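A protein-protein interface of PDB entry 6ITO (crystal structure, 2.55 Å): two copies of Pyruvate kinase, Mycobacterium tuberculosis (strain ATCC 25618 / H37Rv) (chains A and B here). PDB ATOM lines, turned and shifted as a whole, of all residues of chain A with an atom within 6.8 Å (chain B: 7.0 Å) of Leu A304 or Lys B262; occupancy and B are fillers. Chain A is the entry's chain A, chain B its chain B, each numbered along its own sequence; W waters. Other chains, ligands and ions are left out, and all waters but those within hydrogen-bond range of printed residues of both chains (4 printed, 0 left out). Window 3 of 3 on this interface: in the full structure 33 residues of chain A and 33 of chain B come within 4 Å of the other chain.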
ATOM      1  N   LYS A 262     -22.090 -28.587  14.761  1.00  0.00           N
ATOM      2  CA  LYS A 262     -21.764 -29.198  13.456  1.00  0.00           C
ATOM      3  C   LYS A 262     -20.595 -30.166  13.648  1.00  0.00           C
ATOM      4  O   LYS A 262     -20.669 -31.316  13.151  1.00  0.00           O
ATOM      5  CB  LYS A 262     -21.491 -28.121  12.421  1.00  0.00           C
ATOM      6  CG  LYS A 262     -22.746 -27.526  11.816  1.00  0.00           C
ATOM      7  CD  LYS A 262     -22.611 -26.093  11.373  1.00  0.00           C
ATOM      8  CE  LYS A 262     -23.946 -25.492  10.991  1.00  0.00           C
ATOM      9  NZ  LYS A 262     -24.426 -26.037   9.708  1.00  0.00           N
ATOM     10  N   ARG A 269     -20.812 -39.258  14.235  1.00  0.00           N
ATOM     11  CA  ARG A 269     -21.052 -40.124  13.043  1.00  0.00           C
ATOM     12  C   ARG A 269     -19.754 -40.845  12.633  1.00  0.00           C
ATOM     13  O   ARG A 269     -19.847 -41.992  12.185  1.00  0.00           O
ATOM     14  CB  ARG A 269     -21.599 -39.305  11.870  1.00  0.00           C
ATOM     15  CG  ARG A 269     -23.035 -38.845  12.039  1.00  0.00           C
ATOM     16  CD  ARG A 269     -23.497 -38.007  10.872  1.00  0.00           C
ATOM     17  NE  ARG A 269     -23.276 -38.660   9.598  1.00  0.00           N
ATOM     18  CZ  ARG A 269     -22.555 -38.161   8.597  1.00  0.00           C
ATOM     19  NH1 ARG A 269     -21.982 -36.969   8.704  1.00  0.00           N
ATOM     20  NH2 ARG A 269     -22.428 -38.852   7.481  1.00  0.00           N
ATOM     21  N   SER A 297     -35.706 -23.159  10.190  1.00  0.00           N
ATOM     22  CA  SER A 297     -34.322 -23.245   9.621  1.00  0.00           C
ATOM     23  C   SER A 297     -33.440 -24.109  10.532  1.00  0.00           C
ATOM     24  O   SER A 297     -32.645 -24.934  10.011  1.00  0.00           O
ATOM     25  CB  SER A 297     -33.711 -21.839   9.409  1.00  0.00           C
ATOM     26  OG  SER A 297     -32.343 -21.911   9.017  1.00  0.00           O
ATOM     27  N   VAL A 299     -34.057 -26.498  12.632  1.00  0.00           N
ATOM     28  CA  VAL A 299     -34.440 -27.931  12.550  1.00  0.00           C
ATOM     29  C   VAL A 299     -33.941 -28.516  11.212  1.00  0.00           C
ATOM     30  O   VAL A 299     -33.271 -29.556  11.242  1.00  0.00           O
ATOM     31  CB  VAL A 299     -35.961 -28.092  12.729  1.00  0.00           C
ATOM     32  CG1 VAL A 299     -36.427 -29.500  12.407  1.00  0.00           C
ATOM     33  CG2 VAL A 299     -36.408 -27.680  14.130  1.00  0.00           C
ATOM     34  N   ALA A 300     -34.240 -27.869  10.088  1.00  0.00           N
ATOM     35  CA  ALA A 300     -33.808 -28.294   8.730  1.00  0.00           C
ATOM     36  C   ALA A 300     -32.296 -28.471   8.708  1.00  0.00           C
ATOM     37  O   ALA A 300     -31.835 -29.457   8.154  1.00  0.00           O
ATOM     38  CB  ALA A 300     -34.246 -27.291   7.703  1.00  0.00           C
ATOM     39  N   ASN A 301     -31.563 -27.556   9.338  1.00  0.00           N
ATOM     40  CA  ASN A 301     -30.080 -27.500   9.288  1.00  0.00           C
ATOM     41  C   ASN A 301     -29.483 -28.593  10.191  1.00  0.00           C
ATOM     42  O   ASN A 301     -28.421 -29.105   9.846  1.00  0.00           O
ATOM     43  CB  ASN A 301     -29.556 -26.093   9.645  1.00  0.00           C
ATOM     44  CG  ASN A 301     -29.462 -25.182   8.434  1.00  0.00           C
ATOM     45  OD1 ASN A 301     -28.781 -25.518   7.466  1.00  0.00           O
ATOM     46  ND2 ASN A 301     -30.163 -24.050   8.466  1.00  0.00           N
ATOM     47  N   ALA A 302     -30.125 -28.907  11.321  1.00  0.00           N
ATOM     48  CA  ALA A 302     -29.761 -30.053  12.202  1.00  0.00           C
ATOM     49  C   ALA A 302     -29.847 -31.362  11.391  1.00  0.00           C
ATOM     50  O   ALA A 302     -28.951 -32.193  11.514  1.00  0.00           O
ATOM     51  CB  ALA A 302     -30.655 -30.093  13.418  1.00  0.00           C
ATOM     52  N   VAL A 303     -30.848 -31.479  10.527  1.00  0.00           N
ATOM     53  CA  VAL A 303     -31.027 -32.648   9.633  1.00  0.00           C
ATOM     54  C   VAL A 303     -29.856 -32.713   8.647  1.00  0.00           C
ATOM     55  O   VAL A 303     -29.240 -33.762   8.571  1.00  0.00           O
ATOM     56  CB  VAL A 303     -32.388 -32.601   8.927  1.00  0.00           C
ATOM     57  CG1 VAL A 303     -32.467 -33.580   7.781  1.00  0.00           C
ATOM     58  CG2 VAL A 303     -33.514 -32.837   9.916  1.00  0.00           C
ATOM     59  N   LEU A 304     -29.557 -31.621   7.938  1.00  0.00           N
ATOM     60  CA  LEU A 304     -28.494 -31.579   6.884  1.00  0.00           C
ATOM     61  C   LEU A 304     -27.119 -31.706   7.530  1.00  0.00           C
ATOM     62  O   LEU A 304     -26.216 -32.179   6.859  1.00  0.00           O
ATOM     63  CB  LEU A 304     -28.601 -30.281   6.090  1.00  0.00           C
ATOM     64  CG  LEU A 304     -29.916 -30.079   5.338  1.00  0.00           C
ATOM     65  CD1 LEU A 304     -30.110 -28.614   4.969  1.00  0.00           C
ATOM     66  CD2 LEU A 304     -29.979 -30.955   4.101  1.00  0.00           C
ATOM     67  N   ASP A 305     -26.989 -31.285   8.787  1.00  0.00           N
ATOM     68  CA  ASP A 305     -25.760 -31.447   9.614  1.00  0.00           C
ATOM     69  C   ASP A 305     -25.461 -32.929   9.831  1.00  0.00           C
ATOM     70  O   ASP A 305     -24.288 -33.263   9.972  1.00  0.00           O
ATOM     71  CB  ASP A 305     -25.917 -30.787  10.974  1.00  0.00           C
ATOM     72  CG  ASP A 305     -25.735 -29.290  10.959  1.00  0.00           C
ATOM     73  OD1 ASP A 305     -25.236 -28.781   9.942  1.00  0.00           O
ATOM     74  OD2 ASP A 305     -26.108 -28.645  11.973  1.00  0.00           O
ATOM     75  N   GLY A 306     -26.508 -33.762   9.937  1.00  0.00           N
ATOM     76  CA  GLY A 306     -26.412 -35.238  10.024  1.00  0.00           C
ATOM     77  C   GLY A 306     -26.829 -35.774  11.389  1.00  0.00           C
ATOM     78  O   GLY A 306     -26.439 -36.864  11.712  1.00  0.00           O
ATOM     79  N   ALA A 307     -27.610 -35.013  12.142  1.00  0.00           N
ATOM     80  CA  ALA A 307     -28.087 -35.358  13.497  1.00  0.00           C
ATOM     81  C   ALA A 307     -28.947 -36.623  13.428  1.00  0.00           C
ATOM     82  O   ALA A 307     -29.874 -36.680  12.539  1.00  0.00           O
ATOM     83  CB  ALA A 307     -28.861 -34.203  14.081  1.00  0.00           C
ATOM     84  N   VAL A 336     -37.153 -31.890   4.305  1.00  0.00           N
ATOM     85  CA  VAL A 336     -35.700 -31.908   3.986  1.00  0.00           C
ATOM     86  C   VAL A 336     -35.345 -33.244   3.317  1.00  0.00           C
ATOM     87  O   VAL A 336     -34.717 -33.211   2.232  1.00  0.00           O
ATOM     88  CB  VAL A 336     -34.850 -31.654   5.245  1.00  0.00           C
ATOM     89  CG1 VAL A 336     -33.369 -31.790   4.962  1.00  0.00           C
ATOM     90  CG2 VAL A 336     -35.145 -30.298   5.842  1.00  0.00           C
ATOM     91  N   GLU A 337     -35.761 -34.366   3.922  1.00  0.00           N
ATOM     92  CA  GLU A 337     -35.385 -35.750   3.511  1.00  0.00           C
ATOM     93  C   GLU A 337     -36.024 -36.096   2.149  1.00  0.00           C
ATOM     94  O   GLU A 337     -35.376 -36.821   1.354  1.00  0.00           O
ATOM     95  CB  GLU A 337     -35.786 -36.737   4.600  1.00  0.00           C
ATOM     96  CG  GLU A 337     -34.934 -36.632   5.870  1.00  0.00           C
ATOM     97  CD  GLU A 337     -35.456 -37.437   7.063  1.00  0.00           C
ATOM     98  OE1 GLU A 337     -36.561 -38.005   6.954  1.00  0.00           O
ATOM     99  OE2 GLU A 337     -34.760 -37.479   8.105  1.00  0.00           O
ATOM    100  N   ASN A 339     -36.339 -34.094  -0.328  1.00  0.00           N
ATOM    101  CA  ASN A 339     -35.344 -33.506  -1.242  1.00  0.00           C
ATOM    102  C   ASN A 339     -34.103 -34.414  -1.297  1.00  0.00           C
ATOM    103  O   ASN A 339     -33.708 -34.807  -2.408  1.00  0.00           O
ATOM    104  CB  ASN A 339     -34.972 -32.085  -0.832  1.00  0.00           C
ATOM    105  CG  ASN A 339     -33.897 -31.527  -1.718  1.00  0.00           C
ATOM    106  OD1 ASN A 339     -32.722 -31.610  -1.389  1.00  0.00           O
ATOM    107  ND2 ASN A 339     -34.282 -31.072  -2.898  1.00  0.00           N
ATOM    108  N   SER A 340     -33.504 -34.710  -0.138  1.00  0.00           N
ATOM    109  CA  SER A 340     -32.290 -35.562  -0.010  1.00  0.00           C
ATOM    110  C   SER A 340     -32.060 -35.963   1.448  1.00  0.00           C
ATOM    111  O   SER A 340     -32.217 -35.096   2.336  1.00  0.00           O
ATOM    112  CB  SER A 340     -31.073 -34.857  -0.569  1.00  0.00           C
ATOM    113  OG  SER A 340     -29.885 -35.534  -0.200  1.00  0.00           O
ATOM    114  N   THR A 341     -31.646 -37.213   1.665  1.00  0.00           N
ATOM    115  CA  THR A 341     -31.283 -37.779   2.989  1.00  0.00           C
ATOM    116  C   THR A 341     -29.776 -37.628   3.187  1.00  0.00           C
ATOM    117  O   THR A 341     -29.306 -37.947   4.288  1.00  0.00           O
ATOM    118  CB  THR A 341     -31.710 -39.257   3.126  1.00  0.00           C
ATOM    119  OG1 THR A 341     -30.890 -40.046   2.264  1.00  0.00           O
ATOM    120  CG2 THR A 341     -33.161 -39.503   2.779  1.00  0.00           C
ATOM    121  N   ALA A 342     -29.068 -37.133   2.162  1.00  0.00           N
ATOM    122  CA  ALA A 342     -27.588 -36.964   2.115  1.00  0.00           C
ATOM    123  C   ALA A 342     -27.074 -36.238   3.362  1.00  0.00           C
ATOM    124  O   ALA A 342     -27.690 -35.247   3.774  1.00  0.00           O
ATOM    125  CB  ALA A 342     -27.182 -36.218   0.866  1.00  0.00           C
ATOM    126  N   ALA A 343     -25.935 -36.710   3.881  1.00  0.00           N
ATOM    127  CA  ALA A 343     -25.214 -36.178   5.053  1.00  0.00           C
ATOM    128  C   ALA A 343     -23.812 -35.776   4.634  1.00  0.00           C
ATOM    129  O   ALA A 343     -23.277 -36.292   3.665  1.00  0.00           O
ATOM    130  CB  ALA A 343     -25.165 -37.231   6.126  1.00  0.00           C
ATOM    131  N   PRO A 344     -23.129 -34.925   5.407  1.00  0.00           N
ATOM    132  CA  PRO A 344     -21.735 -34.604   5.129  1.00  0.00           C
ATOM    133  C   PRO A 344     -20.887 -35.875   5.098  1.00  0.00           C
ATOM    134  O   PRO A 344     -20.895 -36.656   6.038  1.00  0.00           O
ATOM    135  CB  PRO A 344     -21.330 -33.684   6.290  1.00  0.00           C
ATOM    136  CG  PRO A 344     -22.657 -33.156   6.817  1.00  0.00           C
ATOM    137  CD  PRO A 344     -23.618 -34.305   6.629  1.00  0.00           C
ATOM    138  N   HIS A 390     -26.501 -42.625   6.120  1.00  0.00           N
ATOM    139  CA  HIS A 390     -27.743 -41.943   5.685  1.00  0.00           C
ATOM    140  C   HIS A 390     -28.153 -42.385   4.282  1.00  0.00           C
ATOM    141  O   HIS A 390     -28.230 -41.534   3.417  1.00  0.00           O
ATOM    142  CB  HIS A 390     -27.553 -40.429   5.703  1.00  0.00           C
ATOM    143  CG  HIS A 390     -27.819 -39.777   7.007  1.00  0.00           C
ATOM    144  ND1 HIS A 390     -28.630 -38.662   7.110  1.00  0.00           N
ATOM    145  CD2 HIS A 390     -27.336 -40.029   8.243  1.00  0.00           C
ATOM    146  CE1 HIS A 390     -28.656 -38.269   8.362  1.00  0.00           C
ATOM    147  NE2 HIS A 390     -27.875 -39.112   9.086  1.00  0.00           N
ATOM    148  N   VAL B 243     -34.855 -13.148   0.101  1.00  0.00           N
ATOM    149  CA  VAL B 243     -35.661 -14.280   0.614  1.00  0.00           C
ATOM    150  C   VAL B 243     -36.489 -13.735   1.759  1.00  0.00           C
ATOM    151  O   VAL B 243     -35.922 -13.496   2.836  1.00  0.00           O
ATOM    152  CB  VAL B 243     -34.790 -15.476   1.035  1.00  0.00           C
ATOM    153  CG1 VAL B 243     -35.635 -16.690   1.313  1.00  0.00           C
ATOM    154  CG2 VAL B 243     -33.734 -15.811  -0.008  1.00  0.00           C
ATOM    155  N   VAL B 257     -39.468 -23.602   3.287  1.00  0.00           N
ATOM    156  CA  VAL B 257     -38.734 -22.311   3.170  1.00  0.00           C
ATOM    157  C   VAL B 257     -37.235 -22.566   3.273  1.00  0.00           C
ATOM    158  O   VAL B 257     -36.476 -22.046   2.479  1.00  0.00           O
ATOM    159  CB  VAL B 257     -39.203 -21.286   4.211  1.00  0.00           C
ATOM    160  CG1 VAL B 257     -38.285 -20.074   4.257  1.00  0.00           C
ATOM    161  CG2 VAL B 257     -40.637 -20.864   3.965  1.00  0.00           C
ATOM    162  N   PRO B 258     -36.757 -23.353   4.248  1.00  0.00           N
ATOM    163  CA  PRO B 258     -35.328 -23.564   4.414  1.00  0.00           C
ATOM    164  C   PRO B 258     -34.582 -23.933   3.122  1.00  0.00           C
ATOM    165  O   PRO B 258     -33.498 -23.487   2.939  1.00  0.00           O
ATOM    166  CB  PRO B 258     -35.294 -24.717   5.422  1.00  0.00           C
ATOM    167  CG  PRO B 258     -36.493 -24.457   6.275  1.00  0.00           C
ATOM    168  CD  PRO B 258     -37.544 -24.027   5.285  1.00  0.00           C
ATOM    169  N   LEU B 259     -35.161 -24.769   2.286  1.00  0.00           N
ATOM    170  CA  LEU B 259     -34.484 -25.273   1.063  1.00  0.00           C
ATOM    171  C   LEU B 259     -34.674 -24.262  -0.072  1.00  0.00           C
ATOM    172  O   LEU B 259     -33.839 -24.246  -0.969  1.00  0.00           O
ATOM    173  CB  LEU B 259     -35.045 -26.654   0.679  1.00  0.00           C
ATOM    174  CG  LEU B 259     -34.529 -27.833   1.506  1.00  0.00           C
ATOM    175  CD1 LEU B 259     -35.142 -29.136   1.013  1.00  0.00           C
ATOM    176  CD2 LEU B 259     -33.005 -27.920   1.481  1.00  0.00           C
ATOM    177  N   VAL B 260     -35.768 -23.497  -0.053  1.00  0.00           N
ATOM    178  CA  VAL B 260     -36.032 -22.430  -1.055  1.00  0.00           C
ATOM    179  C   VAL B 260     -34.989 -21.333  -0.841  1.00  0.00           C
ATOM    180  O   VAL B 260     -34.413 -20.879  -1.823  1.00  0.00           O
ATOM    181  CB  VAL B 260     -37.465 -21.873  -0.966  1.00  0.00           C
ATOM    182  CG1 VAL B 260     -37.582 -20.514  -1.656  1.00  0.00           C
ATOM    183  CG2 VAL B 260     -38.498 -22.850  -1.534  1.00  0.00           C
ATOM    184  N   GLN B 261     -34.755 -20.961   0.413  1.00  0.00           N
ATOM    185  CA  GLN B 261     -33.690 -20.024   0.820  1.00  0.00           C
ATOM    186  C   GLN B 261     -32.380 -20.486   0.185  1.00  0.00           C
ATOM    187  O   GLN B 261     -31.727 -19.668  -0.545  1.00  0.00           O
ATOM    188  CB  GLN B 261     -33.578 -19.950   2.355  1.00  0.00           C
ATOM    189  CG  GLN B 261     -32.286 -19.312   2.842  1.00  0.00           C
ATOM    190  CD  GLN B 261     -32.266 -19.067   4.325  1.00  0.00           C
ATOM    191  OE1 GLN B 261     -33.274 -18.715   4.922  1.00  0.00           O
ATOM    192  NE2 GLN B 261     -31.103 -19.264   4.934  1.00  0.00           N
ATOM    193  N   LYS B 262     -31.997 -21.735   0.441  1.00  0.00           N
ATOM    194  CA  LYS B 262     -30.680 -22.273   0.043  1.00  0.00           C
ATOM    195  C   LYS B 262     -30.572 -22.214  -1.477  1.00  0.00           C
ATOM    196  O   LYS B 262     -29.530 -21.754  -1.983  1.00  0.00           O
ATOM    197  CB  LYS B 262     -30.489 -23.674   0.604  1.00  0.00           C
ATOM    198  CG  LYS B 262     -30.050 -23.699   2.056  1.00  0.00           C
ATOM    199  CD  LYS B 262     -30.467 -24.945   2.811  1.00  0.00           C
ATOM    200  CE  LYS B 262     -30.266 -24.805   4.307  1.00  0.00           C
ATOM    201  NZ  LYS B 262     -28.843 -24.848   4.654  1.00  0.00           N
ATOM    202  N   ARG B 263     -31.641 -22.582  -2.167  1.00  0.00           N
ATOM    203  CA  ARG B 263     -31.693 -22.704  -3.642  1.00  0.00           C
ATOM    204  C   ARG B 263     -31.683 -21.288  -4.273  1.00  0.00           C
ATOM    205  O   ARG B 263     -31.184 -21.144  -5.402  1.00  0.00           O
ATOM    206  CB  ARG B 263     -32.917 -23.550  -4.009  1.00  0.00           C
ATOM    207  CG  ARG B 263     -33.237 -23.579  -5.485  1.00  0.00           C
ATOM    208  CD  ARG B 263     -34.651 -24.045  -5.760  1.00  0.00           C
ATOM    209  NE  ARG B 263     -35.050 -23.619  -7.098  1.00  0.00           N
ATOM    210  CZ  ARG B 263     -36.295 -23.621  -7.556  1.00  0.00           C
ATOM    211  NH1 ARG B 263     -37.290 -24.033  -6.781  1.00  0.00           N
ATOM    212  NH2 ARG B 263     -36.541 -23.193  -8.790  1.00  0.00           N
ATOM    213  N   ALA B 264     -32.193 -20.288  -3.561  1.00  0.00           N
ATOM    214  CA  ALA B 264     -32.341 -18.906  -4.054  1.00  0.00           C
ATOM    215  C   ALA B 264     -31.024 -18.170  -3.864  1.00  0.00           C
ATOM    216  O   ALA B 264     -30.685 -17.369  -4.705  1.00  0.00           O
ATOM    217  CB  ALA B 264     -33.475 -18.207  -3.349  1.00  0.00           C
ATOM    218  N   ILE B 265     -30.309 -18.468  -2.794  1.00  0.00           N
ATOM    219  CA  ILE B 265     -28.952 -17.920  -2.530  1.00  0.00           C
ATOM    220  C   ILE B 265     -28.013 -18.429  -3.607  1.00  0.00           C
ATOM    221  O   ILE B 265     -27.230 -17.624  -4.138  1.00  0.00           O
ATOM    222  CB  ILE B 265     -28.472 -18.305  -1.131  1.00  0.00           C
ATOM    223  CG1 ILE B 265     -29.308 -17.610  -0.052  1.00  0.00           C
ATOM    224  CG2 ILE B 265     -26.993 -18.021  -0.986  1.00  0.00           C
ATOM    225  CD1 ILE B 265     -29.023 -18.067   1.358  1.00  0.00           C
ATOM    226  N   GLN B 266     -28.079 -19.718  -3.903  1.00  0.00           N
ATOM    227  CA  GLN B 266     -27.213 -20.394  -4.894  1.00  0.00           C
ATOM    228  C   GLN B 266     -27.485 -19.790  -6.273  1.00  0.00           C
ATOM    229  O   GLN B 266     -26.537 -19.635  -7.039  1.00  0.00           O
ATOM    230  CB  GLN B 266     -27.469 -21.898  -4.891  1.00  0.00           C
ATOM    231  CG  GLN B 266     -26.532 -22.668  -5.801  1.00  0.00           C
ATOM    232  CD  GLN B 266     -25.128 -22.736  -5.264  1.00  0.00           C
ATOM    233  OE1 GLN B 266     -24.892 -22.665  -4.061  1.00  0.00           O
ATOM    234  NE2 GLN B 266     -24.178 -22.907  -6.165  1.00  0.00           N
ATOM    235  N   MET B 267     -28.750 -19.499  -6.570  1.00  0.00           N
ATOM    236  CA  MET B 267     -29.196 -18.934  -7.866  1.00  0.00           C
ATOM    237  C   MET B 267     -28.654 -17.491  -8.006  1.00  0.00           C
ATOM    238  O   MET B 267     -28.158 -17.138  -9.091  1.00  0.00           O
ATOM    239  CB  MET B 267     -30.724 -18.931  -7.947  1.00  0.00           C
ATOM    240  CG  MET B 267     -31.257 -18.517  -9.281  1.00  0.00           C
ATOM    241  SD  MET B 267     -30.843 -19.700 -10.544  1.00  0.00           S
ATOM    242  CE  MET B 267     -32.071 -20.974 -10.222  1.00  0.00           C
ATOM    243  N   ASN B 301     -26.149 -20.247   9.618  1.00  0.00           N
ATOM    244  CA  ASN B 301     -26.467 -21.120   8.459  1.00  0.00           C
ATOM    245  C   ASN B 301     -26.719 -20.262   7.209  1.00  0.00           C
ATOM    246  O   ASN B 301     -26.382 -20.721   6.109  1.00  0.00           O
ATOM    247  CB  ASN B 301     -27.647 -22.070   8.770  1.00  0.00           C
ATOM    248  CG  ASN B 301     -27.194 -23.364   9.428  1.00  0.00           C
ATOM    249  OD1 ASN B 301     -26.365 -24.077   8.877  1.00  0.00           O
ATOM    250  ND2 ASN B 301     -27.692 -23.645  10.626  1.00  0.00           N
ATOM    251  N   ALA B 302     -27.312 -19.079   7.366  1.00  0.00           N
ATOM    252  CA  ALA B 302     -27.463 -18.069   6.279  1.00  0.00           C
ATOM    253  C   ALA B 302     -26.066 -17.677   5.751  1.00  0.00           C
ATOM    254  O   ALA B 302     -25.896 -17.576   4.532  1.00  0.00           O
ATOM    255  CB  ALA B 302     -28.231 -16.872   6.775  1.00  0.00           C
ATOM    256  N   LEU B 304     -23.206 -19.649   5.932  1.00  0.00           N
ATOM    257  CA  LEU B 304     -22.610 -20.844   5.264  1.00  0.00           C
ATOM    258  C   LEU B 304     -23.369 -21.147   3.974  1.00  0.00           C
ATOM    259  O   LEU B 304     -22.775 -21.740   3.087  1.00  0.00           O
ATOM    260  CB  LEU B 304     -22.644 -22.042   6.208  1.00  0.00           C
ATOM    261  CG  LEU B 304     -21.862 -21.876   7.515  1.00  0.00           C
ATOM    262  CD1 LEU B 304     -22.311 -22.910   8.541  1.00  0.00           C
ATOM    263  CD2 LEU B 304     -20.367 -21.980   7.284  1.00  0.00           C
ATOM    264  N   ASP B 305     -24.637 -20.751   3.896  1.00  0.00           N
ATOM    265  CA  ASP B 305     -25.482 -20.852   2.676  1.00  0.00           C
ATOM    266  C   ASP B 305     -24.892 -19.995   1.555  1.00  0.00           C
ATOM    267  O   ASP B 305     -25.067 -20.358   0.393  1.00  0.00           O
ATOM    268  CB  ASP B 305     -26.906 -20.395   2.948  1.00  0.00           C
ATOM    269  CG  ASP B 305     -27.760 -21.433   3.637  1.00  0.00           C
ATOM    270  OD1 ASP B 305     -27.346 -22.581   3.662  1.00  0.00           O
ATOM    271  OD2 ASP B 305     -28.846 -21.065   4.149  1.00  0.00           O
ATOM    272  N   PRO B 344     -20.720 -22.572  -0.726  1.00  0.00           N
ATOM    273  CA  PRO B 344     -20.975 -23.696  -1.621  1.00  0.00           C
ATOM    274  C   PRO B 344     -20.449 -23.390  -3.023  1.00  0.00           C
ATOM    275  O   PRO B 344     -20.794 -22.381  -3.612  1.00  0.00           O
ATOM    276  CB  PRO B 344     -22.509 -23.836  -1.611  1.00  0.00           C
ATOM    277  CG  PRO B 344     -22.940 -23.107  -0.336  1.00  0.00           C
ATOM    278  CD  PRO B 344     -21.942 -21.984  -0.182  1.00  0.00           C
HETATM  279  O   HOH W   1     -29.917 -21.849   6.288  1.00  0.00           O
HETATM  280  O   HOH W   2     -33.051 -22.217   6.165  1.00  0.00           O
HETATM  281  O   HOH W   3     -27.261 -26.144  12.054  1.00  0.00           O
HETATM  282  O   HOH W   4     -30.640 -19.536   7.408  1.00  0.00           O
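The side-chain amide oxygen (OD1) of Asn A301 sits at hydrogen-bond distance from the side-chain amino group (NZ) of Lys B262, 2.9 Å away. The side-chain amino group (NZ) of Lys A262 sits at hydrogen-bond distance from the side-chain amide oxygen (OD1) of Asn B301 (2.9 Å). The side-chain amide oxygen (OD1) of Asn A301 sits close to the side-chain amide oxygen (OD1) of Asn B301 (3.1 Å).
ND2 of Asn A301 is in hydrogen-bond range of O of Ser A297, 3.1 Å away. OD1 of Asp B305 lies within salt-bridge range of NZ of Lys B262, 2.9 Å away. The side-chain carboxylate (OD1) of Asp A305 lies within salt-bridge range of the side-chain amino group (NZ) of Lys A262.
Among the printed residues, pairs that only touch across the chains: Lys A262 with Leu B304 (3.9 Å), Ala A300 with Pro B258 (3.6 Å), Leu A304 with Lys B262 (3.9 Å) and Asn A339 with Leu B259 (3.5 Å).
Of the printed residues of chain B, Leu A304 touches Lys B262 (3.9 Å). Printed residues of chain A within 4 Å of Lys B262: Asn A301 (2.9 Å) and Leu A304 (3.9 Å). Printed residues of chain A within 4 Å of Asn B301: Lys A262 (2.9 Å) and Asn A301 (3.1 Å). Of the printed residues of chain A, Leu B259 touches Asn A339. Printed residues of chain B within 4 Å of Asn A339: Leu B259 (3.5 Å). Printed residues of chain A within 4 Å of Pro B258: Ala A300. Val B243 touches none of the printed residues of chain A. The nearest residue of chain B that does not touch Leu A304 is Leu B259 (4.6 Å). The nearest printed residue of chain B that does not touch Asn A339 is Arg B263 (7.6 Å).
Printed residues of chain A that touch a printed residue of chain B: Lys A262, Ala A300, Asn A301, Leu A304 and Asn A339. Hydrophobic or aromatic side chains of chain A that line the printed part of chain B: Ala A300 and Leu A304. Hydrophobic or aromatic side chains of chain B within 4 Å of the printed part of chain A: Pro B258, Leu B259 and Leu B304. Among the printed residues, 7 pairs touch across the chains.
Lys A262 touches Asn B301, and with the chains exchanged Asn A301 touches Lys B262. Lys A262 touches Leu B304, and with the chains exchanged Leu A304 touches Lys B262. Asn B301 touches its own counterpart, Asn A301. Positions printed for both chains: 262, 301, 302, 304, 305 and 344. Of the 7 pairs that touch across the chains among the printed residues, 5 have their exchanged pair printed and touching as well.
Water W1 lies within hydrogen-bond range of the side-chain carboxylate (OD2) of Asp B305 (2.5 Å), the side-chain amide nitrogen (ND2) of Asn A301 (3.1 Å) and the side-chain amide nitrogen (NE2) of Gln B261 (3.1 Å). Water W4 lies within hydrogen-bond range of the side-chain amide nitrogen (NE2) of Gln B261 (2.5 Å), the side-chain hydroxyl (OG) of Ser A297 (3.3 Å) and the backbone NH (N) of Ala B302 (3.4 Å). Water W3 lies within hydrogen-bond range of the side-chain carboxylate (OD2) of Asp A305 and the side-chain amide nitrogen (ND2) of Asn B301. Water W2 lies within hydrogen-bond range of OG of Ser A297 and O of Pro B258.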
